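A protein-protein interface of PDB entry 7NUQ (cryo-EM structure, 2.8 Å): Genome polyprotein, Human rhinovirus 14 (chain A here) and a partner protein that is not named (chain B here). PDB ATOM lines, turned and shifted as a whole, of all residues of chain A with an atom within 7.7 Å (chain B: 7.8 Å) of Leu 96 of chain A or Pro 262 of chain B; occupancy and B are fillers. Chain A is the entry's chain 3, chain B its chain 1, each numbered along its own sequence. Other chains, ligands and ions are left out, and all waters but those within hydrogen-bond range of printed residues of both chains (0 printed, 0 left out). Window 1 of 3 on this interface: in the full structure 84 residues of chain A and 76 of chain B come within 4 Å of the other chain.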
ATOM      1  N   LEU A  43      23.851   3.961   9.745  1.00  0.00           N
ATOM      2  CA  LEU A  43      22.651   3.948  10.574  1.00  0.00           C
ATOM      3  C   LEU A  43      21.408   3.568   9.782  1.00  0.00           C
ATOM      4  O   LEU A  43      20.427   3.103  10.375  1.00  0.00           O
ATOM      5  CB  LEU A  43      22.446   5.315  11.228  1.00  0.00           C
ATOM      6  CG  LEU A  43      23.567   5.805  12.147  1.00  0.00           C
ATOM      7  CD1 LEU A  43      23.225   7.176  12.707  1.00  0.00           C
ATOM      8  CD2 LEU A  43      23.826   4.817  13.275  1.00  0.00           C
ATOM      9  N   GLU A  45      21.074   1.075   8.098  1.00  0.00           N
ATOM     10  CA  GLU A  45      20.917  -0.372   8.167  1.00  0.00           C
ATOM     11  C   GLU A  45      20.171  -0.782   9.431  1.00  0.00           C
ATOM     12  O   GLU A  45      19.309  -1.667   9.393  1.00  0.00           O
ATOM     13  CB  GLU A  45      22.288  -1.051   8.114  1.00  0.00           C
ATOM     14  CG  GLU A  45      23.128  -0.660   6.909  1.00  0.00           C
ATOM     15  CD  GLU A  45      24.504  -1.295   6.929  1.00  0.00           C
ATOM     16  OE1 GLU A  45      24.730  -2.204   7.754  1.00  0.00           O
ATOM     17  OE2 GLU A  45      25.362  -0.880   6.122  1.00  0.00           O
ATOM     18  N   ILE A  46      20.490  -0.146  10.559  1.00  0.00           N
ATOM     19  CA  ILE A  46      19.843  -0.493  11.820  1.00  0.00           C
ATOM     20  C   ILE A  46      18.504   0.211  11.996  1.00  0.00           C
ATOM     21  O   ILE A  46      17.644  -0.288  12.734  1.00  0.00           O
ATOM     22  CB  ILE A  46      20.759  -0.170  13.012  1.00  0.00           C
ATOM     23  CG1 ILE A  46      21.057   1.331  13.079  1.00  0.00           C
ATOM     24  CG2 ILE A  46      22.054  -0.962  12.908  1.00  0.00           C
ATOM     25  CD1 ILE A  46      21.917   1.730  14.260  1.00  0.00           C
ATOM     26  N   ILE A  47      18.299   1.359  11.343  1.00  0.00           N
ATOM     27  CA  ILE A  47      17.045   2.091  11.497  1.00  0.00           C
ATOM     28  C   ILE A  47      15.868   1.378  10.851  1.00  0.00           C
ATOM     29  O   ILE A  47      14.715   1.716  11.145  1.00  0.00           O
ATOM     30  CB  ILE A  47      17.179   3.510  10.911  1.00  0.00           C
ATOM     31  CG1 ILE A  47      16.015   4.391  11.370  1.00  0.00           C
ATOM     32  CG2 ILE A  47      17.228   3.457   9.392  1.00  0.00           C
ATOM     33  CD1 ILE A  47      16.153   5.845  10.969  1.00  0.00           C
ATOM     34  N   GLN A  48      16.123   0.399   9.986  1.00  0.00           N
ATOM     35  CA  GLN A  48      15.061  -0.331   9.306  1.00  0.00           C
ATOM     36  C   GLN A  48      14.504  -1.481  10.134  1.00  0.00           C
ATOM     37  O   GLN A  48      13.695  -2.258   9.616  1.00  0.00           O
ATOM     38  CB  GLN A  48      15.573  -0.867   7.967  1.00  0.00           C
ATOM     39  CG  GLN A  48      16.092   0.208   7.028  1.00  0.00           C
ATOM     40  CD  GLN A  48      16.709  -0.366   5.768  1.00  0.00           C
ATOM     41  OE1 GLN A  48      16.592  -1.561   5.494  1.00  0.00           O
ATOM     42  NE2 GLN A  48      17.372   0.483   4.993  1.00  0.00           N
ATOM     43  N   VAL A  49      14.909  -1.612  11.393  1.00  0.00           N
ATOM     44  CA  VAL A  49      14.457  -2.703  12.249  1.00  0.00           C
ATOM     45  C   VAL A  49      13.181  -2.275  12.960  1.00  0.00           C
ATOM     46  O   VAL A  49      13.055  -1.125  13.400  1.00  0.00           O
ATOM     47  CB  VAL A  49      15.547  -3.098  13.258  1.00  0.00           C
ATOM     48  CG1 VAL A  49      15.065  -4.236  14.145  1.00  0.00           C
ATOM     49  CG2 VAL A  49      16.826  -3.487  12.528  1.00  0.00           C
ATOM     50  N   ASP A  50      12.233  -3.202  13.075  1.00  0.00           N
ATOM     51  CA  ASP A  50      10.964  -2.907  13.725  1.00  0.00           C
ATOM     52  C   ASP A  50      11.162  -2.713  15.223  1.00  0.00           C
ATOM     53  O   ASP A  50      11.911  -3.457  15.863  1.00  0.00           O
ATOM     54  CB  ASP A  50       9.966  -4.038  13.467  1.00  0.00           C
ATOM     55  CG  ASP A  50       9.485  -4.076  12.030  1.00  0.00           C
ATOM     56  OD1 ASP A  50       9.401  -3.000  11.400  1.00  0.00           O
ATOM     57  OD2 ASP A  50       9.188  -5.182  11.530  1.00  0.00           O
ATOM     58  N   THR A  51      10.490  -1.708  15.779  1.00  0.00           N
ATOM     59  CA  THR A  51      10.515  -1.438  17.208  1.00  0.00           C
ATOM     60  C   THR A  51       9.114  -1.075  17.678  1.00  0.00           C
ATOM     61  O   THR A  51       8.364  -0.390  16.976  1.00  0.00           O
ATOM     62  CB  THR A  51      11.492  -0.306  17.556  1.00  0.00           C
ATOM     63  OG1 THR A  51      11.165   0.865  16.798  1.00  0.00           O
ATOM     64  CG2 THR A  51      12.922  -0.725  17.254  1.00  0.00           C
ATOM     65  N   LEU A  52       8.770  -1.537  18.878  1.00  0.00           N
ATOM     66  CA  LEU A  52       7.436  -1.306  19.414  1.00  0.00           C
ATOM     67  C   LEU A  52       7.195   0.182  19.634  1.00  0.00           C
ATOM     68  O   LEU A  52       8.061   0.903  20.138  1.00  0.00           O
ATOM     69  CB  LEU A  52       7.253  -2.065  20.728  1.00  0.00           C
ATOM     70  CG  LEU A  52       7.287  -3.592  20.636  1.00  0.00           C
ATOM     71  CD1 LEU A  52       7.341  -4.207  22.025  1.00  0.00           C
ATOM     72  CD2 LEU A  52       6.082  -4.113  19.869  1.00  0.00           C
ATOM     73  N   ILE A  87       7.702  11.970  13.344  1.00  0.00           N
ATOM     74  CA  ILE A  87       8.583  10.925  13.864  1.00  0.00           C
ATOM     75  C   ILE A  87       9.600  11.439  14.869  1.00  0.00           C
ATOM     76  O   ILE A  87      10.225  10.630  15.565  1.00  0.00           O
ATOM     77  CB  ILE A  87       9.329  10.220  12.715  1.00  0.00           C
ATOM     78  CG1 ILE A  87      10.160  11.227  11.912  1.00  0.00           C
ATOM     79  CG2 ILE A  87       8.340   9.499  11.808  1.00  0.00           C
ATOM     80  CD1 ILE A  87      10.905  10.611  10.746  1.00  0.00           C
ATOM     81  N   PHE A  92       6.520   8.454  18.595  1.00  0.00           N
ATOM     82  CA  PHE A  92       7.717   7.982  17.914  1.00  0.00           C
ATOM     83  C   PHE A  92       9.001   8.559  18.495  1.00  0.00           C
ATOM     84  O   PHE A  92      10.086   8.088  18.142  1.00  0.00           O
ATOM     85  CB  PHE A  92       7.645   8.327  16.422  1.00  0.00           C
ATOM     86  CG  PHE A  92       6.402   7.829  15.744  1.00  0.00           C
ATOM     87  CD1 PHE A  92       5.283   8.638  15.639  1.00  0.00           C
ATOM     88  CD2 PHE A  92       6.352   6.553  15.207  1.00  0.00           C
ATOM     89  CE1 PHE A  92       4.137   8.184  15.014  1.00  0.00           C
ATOM     90  CE2 PHE A  92       5.210   6.094  14.581  1.00  0.00           C
ATOM     91  CZ  PHE A  92       4.100   6.911  14.485  1.00  0.00           C
ATOM     92  N   LYS A  93       8.904   9.559  19.375  1.00  0.00           N
ATOM     93  CA  LYS A  93      10.103  10.208  19.895  1.00  0.00           C
ATOM     94  C   LYS A  93      11.012   9.211  20.603  1.00  0.00           C
ATOM     95  O   LYS A  93      12.240   9.355  20.582  1.00  0.00           O
ATOM     96  CB  LYS A  93       9.709  11.338  20.847  1.00  0.00           C
ATOM     97  CG  LYS A  93      10.844  12.289  21.185  1.00  0.00           C
ATOM     98  CD  LYS A  93      10.389  13.373  22.148  1.00  0.00           C
ATOM     99  CE  LYS A  93      11.480  14.408  22.382  1.00  0.00           C
ATOM    100  NZ  LYS A  93      11.817  15.159  21.140  1.00  0.00           N
ATOM    101  N   THR A  94      10.429   8.193  21.234  1.00  0.00           N
ATOM    102  CA  THR A  94      11.192   7.233  22.022  1.00  0.00           C
ATOM    103  C   THR A  94      11.601   5.993  21.238  1.00  0.00           C
ATOM    104  O   THR A  94      12.443   5.228  21.721  1.00  0.00           O
ATOM    105  CB  THR A  94      10.384   6.804  23.250  1.00  0.00           C
ATOM    106  OG1 THR A  94       9.109   6.296  22.836  1.00  0.00           O
ATOM    107  CG2 THR A  94      10.177   7.980  24.193  1.00  0.00           C
ATOM    108  N   THR A  95      11.037   5.773  20.054  1.00  0.00           N
ATOM    109  CA  THR A  95      11.379   4.593  19.277  1.00  0.00           C
ATOM    110  C   THR A  95      12.781   4.724  18.687  1.00  0.00           C
ATOM    111  O   THR A  95      13.342   5.817  18.576  1.00  0.00           O
ATOM    112  CB  THR A  95      10.364   4.375  18.153  1.00  0.00           C
ATOM    113  OG1 THR A  95      10.345   5.520  17.290  1.00  0.00           O
ATOM    114  CG2 THR A  95       8.971   4.151  18.726  1.00  0.00           C
ATOM    115  N   LEU A  96      13.350   3.577  18.308  1.00  0.00           N
ATOM    116  CA  LEU A  96      14.678   3.574  17.701  1.00  0.00           C
ATOM    117  C   LEU A  96      14.721   4.473  16.474  1.00  0.00           C
ATOM    118  O   LEU A  96      15.654   5.271  16.309  1.00  0.00           O
ATOM    119  CB  LEU A  96      15.082   2.146  17.332  1.00  0.00           C
ATOM    120  CG  LEU A  96      16.407   1.979  16.581  1.00  0.00           C
ATOM    121  CD1 LEU A  96      17.579   2.454  17.424  1.00  0.00           C
ATOM    122  CD2 LEU A  96      16.598   0.531  16.166  1.00  0.00           C
ATOM    123  N   LEU A  97      13.723   4.357  15.595  1.00  0.00           N
ATOM    124  CA  LEU A  97      13.678   5.206  14.411  1.00  0.00           C
ATOM    125  C   LEU A  97      13.642   6.677  14.803  1.00  0.00           C
ATOM    126  O   LEU A  97      14.387   7.497  14.255  1.00  0.00           O
ATOM    127  CB  LEU A  97      12.465   4.841  13.553  1.00  0.00           C
ATOM    128  CG  LEU A  97      12.307   5.598  12.231  1.00  0.00           C
ATOM    129  CD1 LEU A  97      11.656   4.705  11.187  1.00  0.00           C
ATOM    130  CD2 LEU A  97      11.494   6.874  12.414  1.00  0.00           C
ATOM    131  N   GLY A  98      12.783   7.029  15.760  1.00  0.00           N
ATOM    132  CA  GLY A  98      12.710   8.414  16.196  1.00  0.00           C
ATOM    133  C   GLY A  98      13.989   8.883  16.863  1.00  0.00           C
ATOM    134  O   GLY A  98      14.418  10.022  16.673  1.00  0.00           O
ATOM    135  N   GLU A  99      14.613   8.013  17.661  1.00  0.00           N
ATOM    136  CA  GLU A  99      15.866   8.382  18.311  1.00  0.00           C
ATOM    137  C   GLU A  99      16.963   8.642  17.286  1.00  0.00           C
ATOM    138  O   GLU A  99      17.771   9.563  17.454  1.00  0.00           O
ATOM    139  CB  GLU A  99      16.292   7.289  19.290  1.00  0.00           C
ATOM    140  CG  GLU A  99      15.419   7.190  20.533  1.00  0.00           C
ATOM    141  CD  GLU A  99      15.557   8.394  21.443  1.00  0.00           C
ATOM    142  OE1 GLU A  99      16.419   9.255  21.168  1.00  0.00           O
ATOM    143  OE2 GLU A  99      14.805   8.480  22.437  1.00  0.00           O
ATOM    144  N   ILE A 100      17.010   7.842  16.219  1.00  0.00           N
ATOM    145  CA  ILE A 100      18.020   8.047  15.187  1.00  0.00           C
ATOM    146  C   ILE A 100      17.693   9.283  14.358  1.00  0.00           C
ATOM    147  O   ILE A 100      18.594   9.983  13.882  1.00  0.00           O
ATOM    148  CB  ILE A 100      18.146   6.792  14.306  1.00  0.00           C
ATOM    149  CG1 ILE A 100      18.655   5.610  15.136  1.00  0.00           C
ATOM    150  CG2 ILE A 100      19.073   7.064  13.123  1.00  0.00           C
ATOM    151  CD1 ILE A 100      18.647   4.285  14.397  1.00  0.00           C
ATOM    152  N   VAL A 101      16.403   9.571  14.172  1.00  0.00           N
ATOM    153  CA  VAL A 101      16.010  10.724  13.367  1.00  0.00           C
ATOM    154  C   VAL A 101      16.283  12.023  14.111  1.00  0.00           C
ATOM    155  O   VAL A 101      16.669  13.027  13.500  1.00  0.00           O
ATOM    156  CB  VAL A 101      14.527  10.605  12.962  1.00  0.00           C
ATOM    157  CG1 VAL A 101      14.038  11.903  12.343  1.00  0.00           C
ATOM    158  CG2 VAL A 101      14.333   9.449  11.992  1.00  0.00           C
ATOM    159  N   GLN A 102      16.089  12.032  15.429  1.00  0.00           N
ATOM    160  CA  GLN A 102      16.339  13.230  16.222  1.00  0.00           C
ATOM    161  C   GLN A 102      17.783  13.707  16.131  1.00  0.00           C
ATOM    162  O   GLN A 102      18.042  14.887  16.391  1.00  0.00           O
ATOM    163  CB  GLN A 102      15.973  12.977  17.686  1.00  0.00           C
ATOM    164  CG  GLN A 102      14.476  12.965  17.950  1.00  0.00           C
ATOM    165  CD  GLN A 102      14.139  12.671  19.399  1.00  0.00           C
ATOM    166  OE1 GLN A 102      14.024  13.584  20.217  1.00  0.00           O
ATOM    167  NE2 GLN A 102      13.975  11.395  19.721  1.00  0.00           N
ATOM    168  N   TYR A 103      18.720  12.832  15.772  1.00  0.00           N
ATOM    169  CA  TYR A 103      20.099  13.242  15.539  1.00  0.00           C
ATOM    170  C   TYR A 103      20.287  13.949  14.205  1.00  0.00           C
ATOM    171  O   TYR A 103      21.417  14.328  13.878  1.00  0.00           O
ATOM    172  CB  TYR A 103      21.029  12.026  15.605  1.00  0.00           C
ATOM    173  CG  TYR A 103      21.338  11.565  17.011  1.00  0.00           C
ATOM    174  CD1 TYR A 103      20.657  10.497  17.581  1.00  0.00           C
ATOM    175  CD2 TYR A 103      22.314  12.199  17.770  1.00  0.00           C
ATOM    176  CE1 TYR A 103      20.939  10.074  18.866  1.00  0.00           C
ATOM    177  CE2 TYR A 103      22.601  11.785  19.055  1.00  0.00           C
ATOM    178  CZ  TYR A 103      21.911  10.722  19.598  1.00  0.00           C
ATOM    179  OH  TYR A 103      22.196  10.307  20.878  1.00  0.00           O
ATOM    180  N   ILE A 211       7.366   0.261  14.086  1.00  0.00           N
ATOM    181  CA  ILE A 211       7.785   1.329  13.186  1.00  0.00           C
ATOM    182  C   ILE A 211       9.179   1.000  12.672  1.00  0.00           C
ATOM    183  O   ILE A 211      10.062   0.627  13.453  1.00  0.00           O
ATOM    184  CB  ILE A 211       7.772   2.705  13.880  1.00  0.00           C
ATOM    185  CG1 ILE A 211       8.036   3.826  12.869  1.00  0.00           C
ATOM    186  CG2 ILE A 211       8.806   2.752  14.997  1.00  0.00           C
ATOM    187  CD1 ILE A 211       6.939   3.990  11.835  1.00  0.00           C
ATOM    188  N   THR A 227      16.991  14.550  23.881  1.00  0.00           N
ATOM    189  CA  THR A 227      16.491  13.436  24.674  1.00  0.00           C
ATOM    190  C   THR A 227      17.414  13.063  25.828  1.00  0.00           C
ATOM    191  O   THR A 227      17.050  12.202  26.635  1.00  0.00           O
ATOM    192  CB  THR A 227      16.283  12.206  23.784  1.00  0.00           C
ATOM    193  OG1 THR A 227      17.510  11.879  23.119  1.00  0.00           O
ATOM    194  CG2 THR A 227      15.203  12.475  22.747  1.00  0.00           C
ATOM    195  N   LYS B 118      25.904   9.008  24.417  1.00  0.00           N
ATOM    196  CA  LYS B 118      24.774   8.246  23.896  1.00  0.00           C
ATOM    197  C   LYS B 118      25.082   7.696  22.509  1.00  0.00           C
ATOM    198  O   LYS B 118      24.823   6.519  22.226  1.00  0.00           O
ATOM    199  CB  LYS B 118      23.523   9.122  23.863  1.00  0.00           C
ATOM    200  CG  LYS B 118      22.311   8.442  23.251  1.00  0.00           C
ATOM    201  CD  LYS B 118      21.039   9.226  23.527  1.00  0.00           C
ATOM    202  CE  LYS B 118      19.819   8.516  22.967  1.00  0.00           C
ATOM    203  NZ  LYS B 118      18.556   9.211  23.334  1.00  0.00           N
ATOM    204  N   GLU B 121      27.294   4.803  22.909  1.00  0.00           N
ATOM    205  CA  GLU B 121      26.609   3.673  23.520  1.00  0.00           C
ATOM    206  C   GLU B 121      25.576   3.040  22.597  1.00  0.00           C
ATOM    207  O   GLU B 121      25.100   1.938  22.887  1.00  0.00           O
ATOM    208  CB  GLU B 121      25.927   4.107  24.823  1.00  0.00           C
ATOM    209  CG  GLU B 121      26.861   4.251  26.019  1.00  0.00           C
ATOM    210  CD  GLU B 121      27.256   2.915  26.628  1.00  0.00           C
ATOM    211  OE1 GLU B 121      27.690   2.019  25.876  1.00  0.00           O
ATOM    212  OE2 GLU B 121      27.133   2.764  27.861  1.00  0.00           O
ATOM    213  N   LEU B 122      25.215   3.708  21.499  1.00  0.00           N
ATOM    214  CA  LEU B 122      24.294   3.106  20.542  1.00  0.00           C
ATOM    215  C   LEU B 122      24.784   1.761  20.021  1.00  0.00           C
ATOM    216  O   LEU B 122      23.987   1.015  19.442  1.00  0.00           O
ATOM    217  CB  LEU B 122      24.061   4.049  19.358  1.00  0.00           C
ATOM    218  CG  LEU B 122      23.293   5.345  19.626  1.00  0.00           C
ATOM    219  CD1 LEU B 122      23.101   6.118  18.332  1.00  0.00           C
ATOM    220  CD2 LEU B 122      21.951   5.067  20.288  1.00  0.00           C
ATOM    221  N   PHE B 204      29.557  -1.997  26.265  1.00  0.00           N
ATOM    222  CA  PHE B 204      28.849  -2.702  27.319  1.00  0.00           C
ATOM    223  C   PHE B 204      29.671  -3.925  27.693  1.00  0.00           C
ATOM    224  O   PHE B 204      30.051  -4.714  26.823  1.00  0.00           O
ATOM    225  CB  PHE B 204      27.438  -3.116  26.888  1.00  0.00           C
ATOM    226  CG  PHE B 204      26.454  -1.982  26.870  1.00  0.00           C
ATOM    227  CD1 PHE B 204      26.498  -1.022  25.874  1.00  0.00           C
ATOM    228  CD2 PHE B 204      25.480  -1.879  27.850  1.00  0.00           C
ATOM    229  CE1 PHE B 204      25.590   0.020  25.856  1.00  0.00           C
ATOM    230  CE2 PHE B 204      24.572  -0.840  27.837  1.00  0.00           C
ATOM    231  CZ  PHE B 204      24.626   0.111  26.840  1.00  0.00           C
ATOM    232  N   PRO B 259      24.469  -3.261  17.172  1.00  0.00           N
ATOM    233  CA  PRO B 259      23.702  -2.063  17.529  1.00  0.00           C
ATOM    234  C   PRO B 259      22.743  -2.341  18.675  1.00  0.00           C
ATOM    235  O   PRO B 259      22.152  -3.419  18.776  1.00  0.00           O
ATOM    236  CB  PRO B 259      22.949  -1.723  16.238  1.00  0.00           C
ATOM    237  CG  PRO B 259      22.858  -3.014  15.500  1.00  0.00           C
ATOM    238  CD  PRO B 259      24.103  -3.781  15.843  1.00  0.00           C
ATOM    239  N   ARG B 260      22.591  -1.344  19.541  1.00  0.00           N
ATOM    240  CA  ARG B 260      21.818  -1.477  20.766  1.00  0.00           C
ATOM    241  C   ARG B 260      20.674  -0.471  20.784  1.00  0.00           C
ATOM    242  O   ARG B 260      20.533   0.373  19.895  1.00  0.00           O
ATOM    243  CB  ARG B 260      22.708  -1.279  22.001  1.00  0.00           C
ATOM    244  CG  ARG B 260      23.898  -2.221  22.071  1.00  0.00           C
ATOM    245  CD  ARG B 260      24.696  -1.996  23.343  1.00  0.00           C
ATOM    246  NE  ARG B 260      23.918  -2.295  24.542  1.00  0.00           N
ATOM    247  CZ  ARG B 260      23.777  -3.511  25.062  1.00  0.00           C
ATOM    248  NH1 ARG B 260      24.357  -4.560  24.493  1.00  0.00           N
ATOM    249  NH2 ARG B 260      23.048  -3.679  26.157  1.00  0.00           N
ATOM    250  N   ALA B 261      19.855  -0.575  21.824  1.00  0.00           N
ATOM    251  CA  ALA B 261      18.716   0.321  21.974  1.00  0.00           C
ATOM    252  C   ALA B 261      19.201   1.714  22.361  1.00  0.00           C
ATOM    253  O   ALA B 261      20.193   1.839  23.088  1.00  0.00           O
ATOM    254  CB  ALA B 261      17.755  -0.217  23.031  1.00  0.00           C
ATOM    255  N   PRO B 262      18.540   2.779  21.902  1.00  0.00           N
ATOM    256  CA  PRO B 262      18.986   4.128  22.271  1.00  0.00           C
ATOM    257  C   PRO B 262      18.889   4.363  23.771  1.00  0.00           C
ATOM    258  O   PRO B 262      18.026   3.811  24.457  1.00  0.00           O
ATOM    259  CB  PRO B 262      18.028   5.044  21.499  1.00  0.00           C
ATOM    260  CG  PRO B 262      17.452   4.192  20.419  1.00  0.00           C
ATOM    261  CD  PRO B 262      17.386   2.816  20.991  1.00  0.00           C
ATOM    262  N   ARG B 263      19.796   5.197  24.275  1.00  0.00           N
ATOM    263  CA  ARG B 263      19.776   5.566  25.684  1.00  0.00           C
ATOM    264  C   ARG B 263      18.504   6.338  26.008  1.00  0.00           C
ATOM    265  O   ARG B 263      18.162   7.310  25.326  1.00  0.00           O
ATOM    266  CB  ARG B 263      21.010   6.406  26.019  1.00  0.00           C
ATOM    267  CG  ARG B 263      21.103   6.855  27.471  1.00  0.00           C
ATOM    268  CD  ARG B 263      21.161   5.675  28.423  1.00  0.00           C
ATOM    269  NE  ARG B 263      21.612   6.070  29.753  1.00  0.00           N
ATOM    270  CZ  ARG B 263      21.698   5.243  30.790  1.00  0.00           C
ATOM    271  NH1 ARG B 263      21.356   3.968  30.660  1.00  0.00           N
ATOM    272  NH2 ARG B 263      22.122   5.694  31.962  1.00  0.00           N
ATOM    273  N   ALA B 264      17.802   5.902  27.051  1.00  0.00           N
ATOM    274  CA  ALA B 264      16.568   6.540  27.493  1.00  0.00           C
ATOM    275  C   ALA B 264      16.743   7.314  28.789  1.00  0.00           C
ATOM    276  O   ALA B 264      16.382   8.492  28.861  1.00  0.00           O
ATOM    277  CB  ALA B 264      15.464   5.488  27.664  1.00  0.00           C
ATOM    278  N   LEU B 265      17.299   6.672  29.834  1.00  0.00           N
ATOM    279  CA  LEU B 265      17.553   7.371  31.084  1.00  0.00           C
ATOM    280  C   LEU B 265      18.955   7.972  31.082  1.00  0.00           C
ATOM    281  O   LEU B 265      19.854   7.462  30.406  1.00  0.00           O
ATOM    282  CB  LEU B 265      17.411   6.418  32.267  1.00  0.00           C
ATOM    283  CG  LEU B 265      16.047   5.745  32.455  1.00  0.00           C
ATOM    284  CD1 LEU B 265      15.967   5.086  33.824  1.00  0.00           C
ATOM    285  CD2 LEU B 265      14.904   6.734  32.269  1.00  0.00           C
ATOM    286  N   TYR B 267      22.684   9.464  32.807  1.00  0.00           N
ATOM    287  CA  TYR B 267      23.765   8.816  33.532  1.00  0.00           C
ATOM    288  C   TYR B 267      24.061   9.541  34.842  1.00  0.00           C
ATOM    289  O   TYR B 267      23.633  10.674  35.076  1.00  0.00           O
ATOM    290  CB  TYR B 267      25.027   8.758  32.672  1.00  0.00           C
ATOM    291  CG  TYR B 267      24.960   7.726  31.577  1.00  0.00           C
ATOM    292  CD1 TYR B 267      24.637   8.085  30.277  1.00  0.00           C
ATOM    293  CD2 TYR B 267      25.208   6.386  31.846  1.00  0.00           C
ATOM    294  CE1 TYR B 267      24.572   7.141  29.272  1.00  0.00           C
ATOM    295  CE2 TYR B 267      25.144   5.432  30.847  1.00  0.00           C
ATOM    296  CZ  TYR B 267      24.826   5.816  29.561  1.00  0.00           C
ATOM    297  OH  TYR B 267      24.759   4.875  28.561  1.00  0.00           O
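Of the 24 printed residues of chain A, 5 touch a printed residue of chain B. Hydrophobic or aromatic side chains of chain A within 4 Å of the printed part of chain B: Ile 46, Leu 96 and Tyr 103. Of the 12 printed residues of chain B, 3 touch a printed residue of chain A. Printed residues of chain B that touch a printed residue of chain A: Lys 118, Pro 259 and Pro 262. Hydrophobic or aromatic side chains of chain B that line the printed part of chain A: Pro 259 and Pro 262. Among the printed residues, 6 pairs touch across the chains.
No residue of chain A comes within 4 Å of Ala 261 of chain B. Of the printed residues of chain A, Lys 118 of chain B touches Glu 99, Tyr 103 and Thr 227. Of the printed residues of chain B, Glu 99 of chain A touches Lys 118 and Pro 262. Printed residues of chain B within 4 Å of Thr 227 of chain A: Lys 118. Leu 265 of chain B touches none of the printed residues of chain A. Leu 122 of chain B touches none of the printed residues of chain A.
NZ of Lys 118 of chain B sits at hydrogen-bond distance from O of Arg 263 of chain B, 2.8 Å away. OE1 of Glu 99 of chain A sits at hydrogen-bond distance from OG1 of Thr 227 of chain A, at 3.4 Å.
NZ of Lys 118 of chain B is in salt-bridge range of OE1 of Glu 99 of chain A, at 3.0 Å. The side-chain amino group of Lys 118 of chain B sits at hydrogen-bond distance from the side-chain hydroxyl of Thr 227 of chain A (2.9 Å).
Among the printed residues, merely in contact across the chains: Tyr 103 of chain A with Lys 118 of chain B (3.0 Å), Ile 46 of chain A with Pro 259 of chain B (3.4 Å), Leu 96 of chain A with Pro 262 of chain B (3.5 Å) and Glu 99 of chain A with Pro 262 of chain B (3.5 Å).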
